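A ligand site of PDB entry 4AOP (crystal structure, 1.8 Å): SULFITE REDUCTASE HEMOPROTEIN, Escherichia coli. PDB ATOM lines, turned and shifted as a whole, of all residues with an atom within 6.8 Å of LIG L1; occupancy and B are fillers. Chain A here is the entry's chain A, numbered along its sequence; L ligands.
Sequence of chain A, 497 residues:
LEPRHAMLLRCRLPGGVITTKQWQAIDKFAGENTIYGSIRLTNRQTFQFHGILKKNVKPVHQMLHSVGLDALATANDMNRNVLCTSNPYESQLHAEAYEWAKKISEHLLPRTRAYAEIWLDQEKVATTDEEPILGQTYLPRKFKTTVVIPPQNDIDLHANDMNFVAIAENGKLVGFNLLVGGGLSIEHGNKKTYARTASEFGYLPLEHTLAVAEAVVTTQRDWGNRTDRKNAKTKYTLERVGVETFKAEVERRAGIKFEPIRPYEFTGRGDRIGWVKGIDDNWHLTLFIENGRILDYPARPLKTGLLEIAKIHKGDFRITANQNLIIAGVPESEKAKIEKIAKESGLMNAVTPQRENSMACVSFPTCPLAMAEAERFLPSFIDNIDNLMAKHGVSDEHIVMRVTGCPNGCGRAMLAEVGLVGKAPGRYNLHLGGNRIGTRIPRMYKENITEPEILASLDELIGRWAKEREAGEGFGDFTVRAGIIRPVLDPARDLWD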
ATOM      1  N   ALA A 360     -11.774 -16.881  13.848  1.00  0.00           N
ATOM      2  CA  ALA A 360     -13.167 -16.875  13.431  1.00  0.00           C
ATOM      3  C   ALA A 360     -13.314 -15.877  12.283  1.00  0.00           C
ATOM      4  O   ALA A 360     -12.492 -14.965  12.153  1.00  0.00           O
ATOM      5  CB  ALA A 360     -14.071 -16.467  14.607  1.00  0.00           C
ATOM      6  N   CYS A 361     -14.329 -16.082  11.440  1.00  0.00           N
ATOM      7  CA  CYS A 361     -14.615 -15.160  10.346  1.00  0.00           C
ATOM      8  C   CYS A 361     -15.516 -14.026  10.877  1.00  0.00           C
ATOM      9  O   CYS A 361     -16.024 -14.108  12.016  1.00  0.00           O
ATOM     10  CB  CYS A 361     -15.346 -15.876   9.203  1.00  0.00           C
ATOM     11  SG  CYS A 361     -17.056 -16.305   9.647  1.00  0.00           S
ATOM     12  N   VAL A 362     -15.749 -13.013  10.050  1.00  0.00           N
ATOM     13  CA  VAL A 362     -16.591 -11.864  10.398  1.00  0.00           C
ATOM     14  C   VAL A 362     -18.023 -12.268  10.793  1.00  0.00           C
ATOM     15  O   VAL A 362     -18.463 -11.976  11.901  1.00  0.00           O
ATOM     16  CB  VAL A 362     -16.622 -10.842   9.247  1.00  0.00           C
ATOM     17  CG1 VAL A 362     -17.568  -9.728   9.597  1.00  0.00           C
ATOM     18  CG2 VAL A 362     -15.241 -10.258   9.030  1.00  0.00           C
ATOM     19  N   SER A 363     -18.722 -12.985   9.905  1.00  0.00           N
ATOM     20  CA  SER A 363     -20.102 -13.413  10.179  1.00  0.00           C
ATOM     21  C   SER A 363     -21.017 -12.220  10.516  1.00  0.00           C
ATOM     22  O   SER A 363     -20.824 -11.136   9.950  1.00  0.00           O
ATOM     23  CB  SER A 363     -20.132 -14.466  11.300  1.00  0.00           C
ATOM     24  OG  SER A 363     -21.410 -15.086  11.374  1.00  0.00           O
ATOM     25  N   PHE A 364     -22.011 -12.424  11.395  1.00  0.00           N
ATOM     26  CA  PHE A 364     -22.913 -11.340  11.810  1.00  0.00           C
ATOM     27  C   PHE A 364     -22.062 -10.296  12.521  1.00  0.00           C
ATOM     28  O   PHE A 364     -21.132 -10.673  13.240  1.00  0.00           O
ATOM     29  CB  PHE A 364     -23.978 -11.850  12.780  1.00  0.00           C
ATOM     30  CG  PHE A 364     -24.845 -12.946  12.225  1.00  0.00           C
ATOM     31  CD1 PHE A 364     -25.716 -12.688  11.164  1.00  0.00           C
ATOM     32  CD2 PHE A 364     -24.776 -14.222  12.743  1.00  0.00           C
ATOM     33  CE1 PHE A 364     -26.509 -13.684  10.649  1.00  0.00           C
ATOM     34  CE2 PHE A 364     -25.592 -15.247  12.209  1.00  0.00           C
ATOM     35  CZ  PHE A 364     -26.440 -14.961  11.167  1.00  0.00           C
ATOM     36  N   CYS A 367     -22.006  -9.862   7.627  1.00  0.00           N
ATOM     37  CA  CYS A 367     -22.005 -10.810   6.521  1.00  0.00           C
ATOM     38  C   CYS A 367     -23.403 -11.246   6.119  1.00  0.00           C
ATOM     39  O   CYS A 367     -24.133 -11.842   6.892  1.00  0.00           O
ATOM     40  CB  CYS A 367     -21.161 -12.039   6.823  1.00  0.00           C
ATOM     41  SG  CYS A 367     -21.065 -13.093   5.360  1.00  0.00           S
ATOM     42  N   PRO A 368     -23.762 -11.033   4.860  1.00  0.00           N
ATOM     43  CA  PRO A 368     -25.101 -11.440   4.432  1.00  0.00           C
ATOM     44  C   PRO A 368     -25.306 -12.948   4.296  1.00  0.00           C
ATOM     45  O   PRO A 368     -26.444 -13.412   4.199  1.00  0.00           O
ATOM     46  CB  PRO A 368     -25.247 -10.723   3.089  1.00  0.00           C
ATOM     47  CG  PRO A 368     -23.850 -10.690   2.562  1.00  0.00           C
ATOM     48  CD  PRO A 368     -23.056 -10.317   3.781  1.00  0.00           C
ATOM     49  N   LEU A 369     -24.225 -13.722   4.325  1.00  0.00           N
ATOM     50  CA  LEU A 369     -24.320 -15.161   4.162  1.00  0.00           C
ATOM     51  C   LEU A 369     -24.221 -15.926   5.465  1.00  0.00           C
ATOM     52  O   LEU A 369     -24.326 -17.147   5.476  1.00  0.00           O
ATOM     53  CB  LEU A 369     -23.217 -15.645   3.198  1.00  0.00           C
ATOM     54  CG  LEU A 369     -23.114 -14.824   1.909  1.00  0.00           C
ATOM     55  CD1 LEU A 369     -21.977 -15.335   1.039  1.00  0.00           C
ATOM     56  CD2 LEU A 369     -24.442 -14.874   1.148  1.00  0.00           C
ATOM     57  N   ALA A 370     -24.067 -15.198   6.566  1.00  0.00           N
ATOM     58  CA  ALA A 370     -23.898 -15.810   7.881  1.00  0.00           C
ATOM     59  C   ALA A 370     -25.053 -16.709   8.313  1.00  0.00           C
ATOM     60  O   ALA A 370     -26.220 -16.381   8.098  1.00  0.00           O
ATOM     61  CB  ALA A 370     -23.655 -14.722   8.919  1.00  0.00           C
ATOM     62  N   MET A 371     -24.712 -17.853   8.904  1.00  0.00           N
ATOM     63  CA  MET A 371     -25.700 -18.795   9.417  1.00  0.00           C
ATOM     64  C   MET A 371     -25.602 -18.818  10.946  1.00  0.00           C
ATOM     65  O   MET A 371     -26.602 -18.940  11.634  1.00  0.00           O
ATOM     66  CB  MET A 371     -25.494 -20.183   8.842  1.00  0.00           C
ATOM     67  CG  MET A 371     -25.804 -20.305   7.348  1.00  0.00           C
ATOM     68  SD  MET A 371     -25.296 -21.946   6.744  1.00  0.00           S
ATOM     69  CE  MET A 371     -25.896 -21.972   5.020  1.00  0.00           C
ATOM     70  N   ALA A 372     -24.392 -18.676  11.471  1.00  0.00           N
ATOM     71  CA  ALA A 372     -24.184 -18.678  12.915  1.00  0.00           C
ATOM     72  C   ALA A 372     -23.102 -17.650  13.220  1.00  0.00           C
ATOM     73  O   ALA A 372     -22.321 -17.298  12.346  1.00  0.00           O
ATOM     74  CB  ALA A 372     -23.746 -20.053  13.392  1.00  0.00           C
ATOM     75  N   ALA A 374     -19.667 -15.971  14.534  1.00  0.00           N
ATOM     76  CA  ALA A 374     -18.304 -16.491  14.515  1.00  0.00           C
ATOM     77  C   ALA A 374     -17.457 -15.517  15.315  1.00  0.00           C
ATOM     78  O   ALA A 374     -17.148 -15.766  16.480  1.00  0.00           O
ATOM     79  CB  ALA A 374     -17.809 -16.630  13.113  1.00  0.00           C
ATOM     80  N   VAL A 403     -13.665 -21.173  13.992  1.00  0.00           N
ATOM     81  CA  VAL A 403     -15.096 -21.116  13.839  1.00  0.00           C
ATOM     82  C   VAL A 403     -15.390 -20.341  12.578  1.00  0.00           C
ATOM     83  O   VAL A 403     -14.890 -19.225  12.387  1.00  0.00           O
ATOM     84  CB  VAL A 403     -15.736 -20.358  15.032  1.00  0.00           C
ATOM     85  CG1 VAL A 403     -17.266 -20.387  14.941  1.00  0.00           C
ATOM     86  CG2 VAL A 403     -15.250 -20.957  16.376  1.00  0.00           C
ATOM     87  N   THR A 404     -16.165 -20.939  11.701  1.00  0.00           N
ATOM     88  CA  THR A 404     -16.526 -20.265  10.473  1.00  0.00           C
ATOM     89  C   THR A 404     -18.065 -20.133  10.501  1.00  0.00           C
ATOM     90  O   THR A 404     -18.755 -21.053  10.938  1.00  0.00           O
ATOM     91  CB  THR A 404     -15.949 -21.013   9.242  1.00  0.00           C
ATOM     92  OG1 THR A 404     -16.012 -20.161   8.098  1.00  0.00           O
ATOM     93  CG2 THR A 404     -16.630 -22.327   8.971  1.00  0.00           C
ATOM     94  N   GLY A 405     -18.559 -18.942  10.170  1.00  0.00           N
ATOM     95  CA  GLY A 405     -19.990 -18.648  10.186  1.00  0.00           C
ATOM     96  C   GLY A 405     -20.937 -19.388   9.254  1.00  0.00           C
ATOM     97  O   GLY A 405     -22.144 -19.447   9.502  1.00  0.00           O
ATOM     98  N   CYS A 406     -20.401 -19.920   8.164  1.00  0.00           N
ATOM     99  CA  CYS A 406     -21.206 -20.666   7.216  1.00  0.00           C
ATOM    100  C   CYS A 406     -20.179 -21.528   6.502  1.00  0.00           C
ATOM    101  O   CYS A 406     -18.972 -21.284   6.632  1.00  0.00           O
ATOM    102  CB  CYS A 406     -21.976 -19.739   6.280  1.00  0.00           C
ATOM    103  SG  CYS A 406     -21.099 -19.002   4.870  1.00  0.00           S
ATOM    104  N   PRO A 407     -20.616 -22.527   5.712  1.00  0.00           N
ATOM    105  CA  PRO A 407     -19.689 -23.407   5.016  1.00  0.00           C
ATOM    106  C   PRO A 407     -18.758 -22.807   3.955  1.00  0.00           C
ATOM    107  O   PRO A 407     -17.866 -23.503   3.452  1.00  0.00           O
ATOM    108  CB  PRO A 407     -20.604 -24.512   4.482  1.00  0.00           C
ATOM    109  CG  PRO A 407     -21.846 -23.751   4.145  1.00  0.00           C
ATOM    110  CD  PRO A 407     -22.014 -22.847   5.350  1.00  0.00           C
ATOM    111  N   ASN A 408     -18.961 -21.533   3.587  1.00  0.00           N
ATOM    112  CA  ASN A 408     -18.079 -20.854   2.624  1.00  0.00           C
ATOM    113  C   ASN A 408     -16.648 -20.969   3.174  1.00  0.00           C
ATOM    114  O   ASN A 408     -15.673 -20.927   2.420  1.00  0.00           O
ATOM    115  CB  ASN A 408     -18.481 -19.391   2.432  1.00  0.00           C
ATOM    116  CG  ASN A 408     -19.658 -19.225   1.488  1.00  0.00           C
ATOM    117  OD1 ASN A 408     -19.895 -20.080   0.635  1.00  0.00           O
ATOM    118  ND2 ASN A 408     -20.391 -18.136   1.614  1.00  0.00           N
ATOM    119  N   GLY A 409     -16.549 -21.052   4.487  1.00  0.00           N
ATOM    120  CA  GLY A 409     -15.280 -21.295   5.142  1.00  0.00           C
ATOM    121  C   GLY A 409     -14.208 -20.260   5.312  1.00  0.00           C
ATOM    122  O   GLY A 409     -13.044 -20.646   5.518  1.00  0.00           O
ATOM    123  N   CYS A 410     -14.585 -18.982   5.377  1.00  0.00           N
ATOM    124  CA  CYS A 410     -13.633 -17.894   5.549  1.00  0.00           C
ATOM    125  C   CYS A 410     -12.777 -18.007   6.816  1.00  0.00           C
ATOM    126  O   CYS A 410     -11.628 -17.594   6.824  1.00  0.00           O
ATOM    127  CB  CYS A 410     -14.367 -16.563   5.529  1.00  0.00           C
ATOM    128  SG  CYS A 410     -15.527 -16.493   4.137  1.00  0.00           S
ATOM    129  N   GLY A 411     -13.325 -18.563   7.891  1.00  0.00           N
ATOM    130  CA  GLY A 411     -12.568 -18.709   9.114  1.00  0.00           C
ATOM    131  C   GLY A 411     -11.539 -19.840   9.091  1.00  0.00           C
ATOM    132  O   GLY A 411     -10.848 -20.070  10.085  1.00  0.00           O
HETATM  133 FE1  LIG L   1     -18.115 -16.192   7.715  1.00  0.00          FE
HETATM  134 FE2  LIG L   1     -19.656 -14.765   5.967  1.00  0.00          FE
HETATM  135 FE3  LIG L   1     -19.754 -17.452   5.796  1.00  0.00          FE
HETATM  136 FE4  LIG L   1     -17.440 -16.105   5.175  1.00  0.00          FE
HETATM  137  S1  LIG L   1     -19.408 -15.960   4.103  1.00  0.00           S
HETATM  138  S2  LIG L   1     -17.656 -18.032   6.315  1.00  0.00           S
HETATM  139  S3  LIG L   1     -17.546 -14.400   6.753  1.00  0.00           S
HETATM  140  S4  LIG L   1     -20.391 -16.160   7.568  1.00  0.00           S
HETATM  141 FE1  LG2 L   2     -14.378 -14.882   2.321  1.00  0.00          FE
HETATM  142  C1  LG2 L   2     -17.370 -14.381   0.818  1.00  0.00           C
HETATM  143  C2  LG2 L   2     -15.247 -12.444   4.734  1.00  0.00           C
HETATM  144  C3  LG2 L   2     -11.354 -15.204   3.685  1.00  0.00           C
HETATM  145  C4  LG2 L   2     -14.186 -18.155   1.146  1.00  0.00           C
HETATM  146  N1  LG2 L   2     -15.943 -13.568   2.679  1.00  0.00           N
HETATM  147  C5  LG2 L   2     -17.027 -13.426   1.745  1.00  0.00           C
HETATM  148  C6  LG2 L   2     -17.822 -12.161   2.115  1.00  0.00           C
HETATM  149  C7  LG2 L   2     -17.192 -11.028   1.177  1.00  0.00           C
HETATM  150  C8  LG2 L   2     -19.312 -12.363   1.909  1.00  0.00           C
HETATM  151  C9  LG2 L   2     -19.946 -11.903   0.598  1.00  0.00           C
HETATM  152  O1  LG2 L   2     -19.688 -12.512  -0.465  1.00  0.00           O
HETATM  153  O2  LG2 L   2     -20.689 -10.914   0.617  1.00  0.00           O
HETATM  154  C10 LG2 L   2     -17.525 -12.066   3.593  1.00  0.00           C
HETATM  155  C11 LG2 L   2     -17.488 -10.673   4.069  1.00  0.00           C
HETATM  156  C12 LG2 L   2     -17.999 -10.635   5.511  1.00  0.00           C
HETATM  157  C13 LG2 L   2     -17.905  -9.247   6.137  1.00  0.00           C
HETATM  158  O3  LG2 L   2     -18.931  -8.759   6.641  1.00  0.00           O
HETATM  159  O4  LG2 L   2     -16.809  -8.667   6.142  1.00  0.00           O
HETATM  160  C14 LG2 L   2     -16.182 -12.733   3.762  1.00  0.00           C
HETATM  161  N2  LG2 L   2     -13.415 -13.891   3.886  1.00  0.00           N
HETATM  162  C15 LG2 L   2     -13.927 -12.946   4.749  1.00  0.00           C
HETATM  163  C16 LG2 L   2     -12.798 -12.595   5.694  1.00  0.00           C
HETATM  164  C17 LG2 L   2     -12.901 -11.054   5.958  1.00  0.00           C
HETATM  165  C18 LG2 L   2     -12.959 -13.551   6.966  1.00  0.00           C
HETATM  166  C19 LG2 L   2     -12.178 -12.994   8.154  1.00  0.00           C
HETATM  167  O5  LG2 L   2     -12.747 -12.846   9.235  1.00  0.00           O
HETATM  168  O6  LG2 L   2     -10.971 -12.696   7.981  1.00  0.00           O
HETATM  169  C20 LG2 L   2     -11.555 -12.853   4.770  1.00  0.00           C
HETATM  170  C21 LG2 L   2     -11.511 -11.785   3.764  1.00  0.00           C
HETATM  171  C22 LG2 L   2     -10.162 -12.132   3.208  1.00  0.00           C
HETATM  172  C23 LG2 L   2      -9.670 -11.082   2.257  1.00  0.00           C
HETATM  173  O7  LG2 L   2      -9.095 -10.089   2.729  1.00  0.00           O
HETATM  174  O8  LG2 L   2      -9.869 -11.244   1.043  1.00  0.00           O
HETATM  175  C24 LG2 L   2     -12.070 -14.087   4.106  1.00  0.00           C
HETATM  176  N3  LG2 L   2     -13.028 -16.453   2.444  1.00  0.00           N
HETATM  177  C25 LG2 L   2     -11.803 -16.315   2.988  1.00  0.00           C
HETATM  178  C26 LG2 L   2     -11.265 -17.689   3.130  1.00  0.00           C
HETATM  179  C27 LG2 L   2      -9.907 -17.999   3.720  1.00  0.00           C
HETATM  180  C28 LG2 L   2      -8.657 -17.549   2.972  1.00  0.00           C
HETATM  181  O9  LG2 L   2      -8.759 -17.063   1.831  1.00  0.00           O
HETATM  182  O10 LG2 L   2      -7.556 -17.669   3.531  1.00  0.00           O
HETATM  183  C29 LG2 L   2     -12.036 -18.521   2.420  1.00  0.00           C
HETATM  184  C30 LG2 L   2     -11.840 -19.979   2.337  1.00  0.00           C
HETATM  185  C31 LG2 L   2     -10.866 -20.539   1.302  1.00  0.00           C
HETATM  186  C32 LG2 L   2     -11.492 -20.682  -0.064  1.00  0.00           C
HETATM  187  O11 LG2 L   2     -11.626 -19.679  -0.770  1.00  0.00           O
HETATM  188  O12 LG2 L   2     -11.858 -21.810  -0.434  1.00  0.00           O
HETATM  189  C33 LG2 L   2     -13.112 -17.691   1.915  1.00  0.00           C
HETATM  190  N4  LG2 L   2     -15.489 -16.088   1.091  1.00  0.00           N
HETATM  191  C34 LG2 L   2     -15.255 -17.383   0.762  1.00  0.00           C
HETATM  192  C35 LG2 L   2     -16.345 -17.791  -0.131  1.00  0.00           C
HETATM  193  C36 LG2 L   2     -16.519 -19.137  -0.748  1.00  0.00           C
HETATM  194  C37 LG2 L   2     -15.718 -19.093  -2.029  1.00  0.00           C
HETATM  195  C38 LG2 L   2     -15.878 -20.341  -2.871  1.00  0.00           C
HETATM  196  O13 LG2 L   2     -14.947 -20.662  -3.636  1.00  0.00           O
HETATM  197  O14 LG2 L   2     -16.945 -20.984  -2.790  1.00  0.00           O
HETATM  198  C39 LG2 L   2     -17.214 -16.733  -0.225  1.00  0.00           C
HETATM  199  C40 LG2 L   2     -18.531 -16.602  -0.996  1.00  0.00           C
HETATM  200  C41 LG2 L   2     -18.395 -16.368  -2.479  1.00  0.00           C
HETATM  201  O15 LG2 L   2     -17.438 -15.714  -2.929  1.00  0.00           O
HETATM  202  O16 LG2 L   2     -19.280 -16.840  -3.210  1.00  0.00           O
HETATM  203  C42 LG2 L   2     -16.719 -15.608   0.586  1.00  0.00           C
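Merely in contact with LIG L1: Ala 370 (3.5 Å), Gly 405 (3.6 Å) and Leu 369 (3.9 Å). Hydrophobic or aromatic side chains within 4 Å of LIG L1: Leu 369 and Ala 370. The nearest printed residue that does not touch LIG L1 is Val 362 (4.003 Å).
SG of Cys 361 sits close to N of Ser 363 (3.7 Å). The backbone NH (N) of Cys 410 lies within hydrogen-bond range of the side-chain hydroxyl (OG1) of Thr 404. OG1 of Thr 404 sits close to O of Cys 406 (3.5 Å). SG of Cys 406 lies close to ND2 of Asn 408 (3.4 Å). The side-chain sulfur (SG) of Cys 406 sits close to the backbone carbonyl oxygen (O) of Leu 369 (3.8 Å). N of Leu 369 sits close to SG of Cys 367 (3.4 Å). OG1 of Thr 404 sits at hydrogen-bond distance from N of Gly 411 (3.1 Å). The backbone NH (N) of Ala 372 is in hydrogen-bond range of the backbone carbonyl oxygen (O) of Gly 405.
The side-chain sulfur (SG) of Cys 361 binds an iron atom (FE1) of LIG L1 (2.2 Å). N of Cys 410 sits close to S2 of LIG L1 (3.3 Å). SG of Cys 410 is bound to FE4 of LIG L1 (2.2 Å). An iron atom (FE3) of LIG L1 is bound by the side-chain sulfur of Cys 406, at 2.3 Å. The side-chain sulfur of Cys 367 is bound to an iron atom (FE2) of LIG L1. OG1 of Thr 404 lies close to S2 of LIG L1 (3.2 Å). The side-chain amide nitrogen (ND2) of Asn 408 lies close to a sulfur (S1) of LIG L1, 3.4 Å away. The backbone NH (N) of Ser 363 sits close to a sulfur (S3) of LIG L1 (3.6 Å). The backbone NH (N) of Gly 409 sits close to a sulfur (S2) of LIG L1 (3.7 Å). SG of Cys 410 is bound to FE1 of LG2 L2 (2.7 Å). An oxygen (O3) of LG2 L2 lies within hydrogen-bond range of the backbone NH (N) of Cys 367. O5 of LG2 L2 sits at hydrogen-bond distance from N of Val 362 (3.1 Å).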
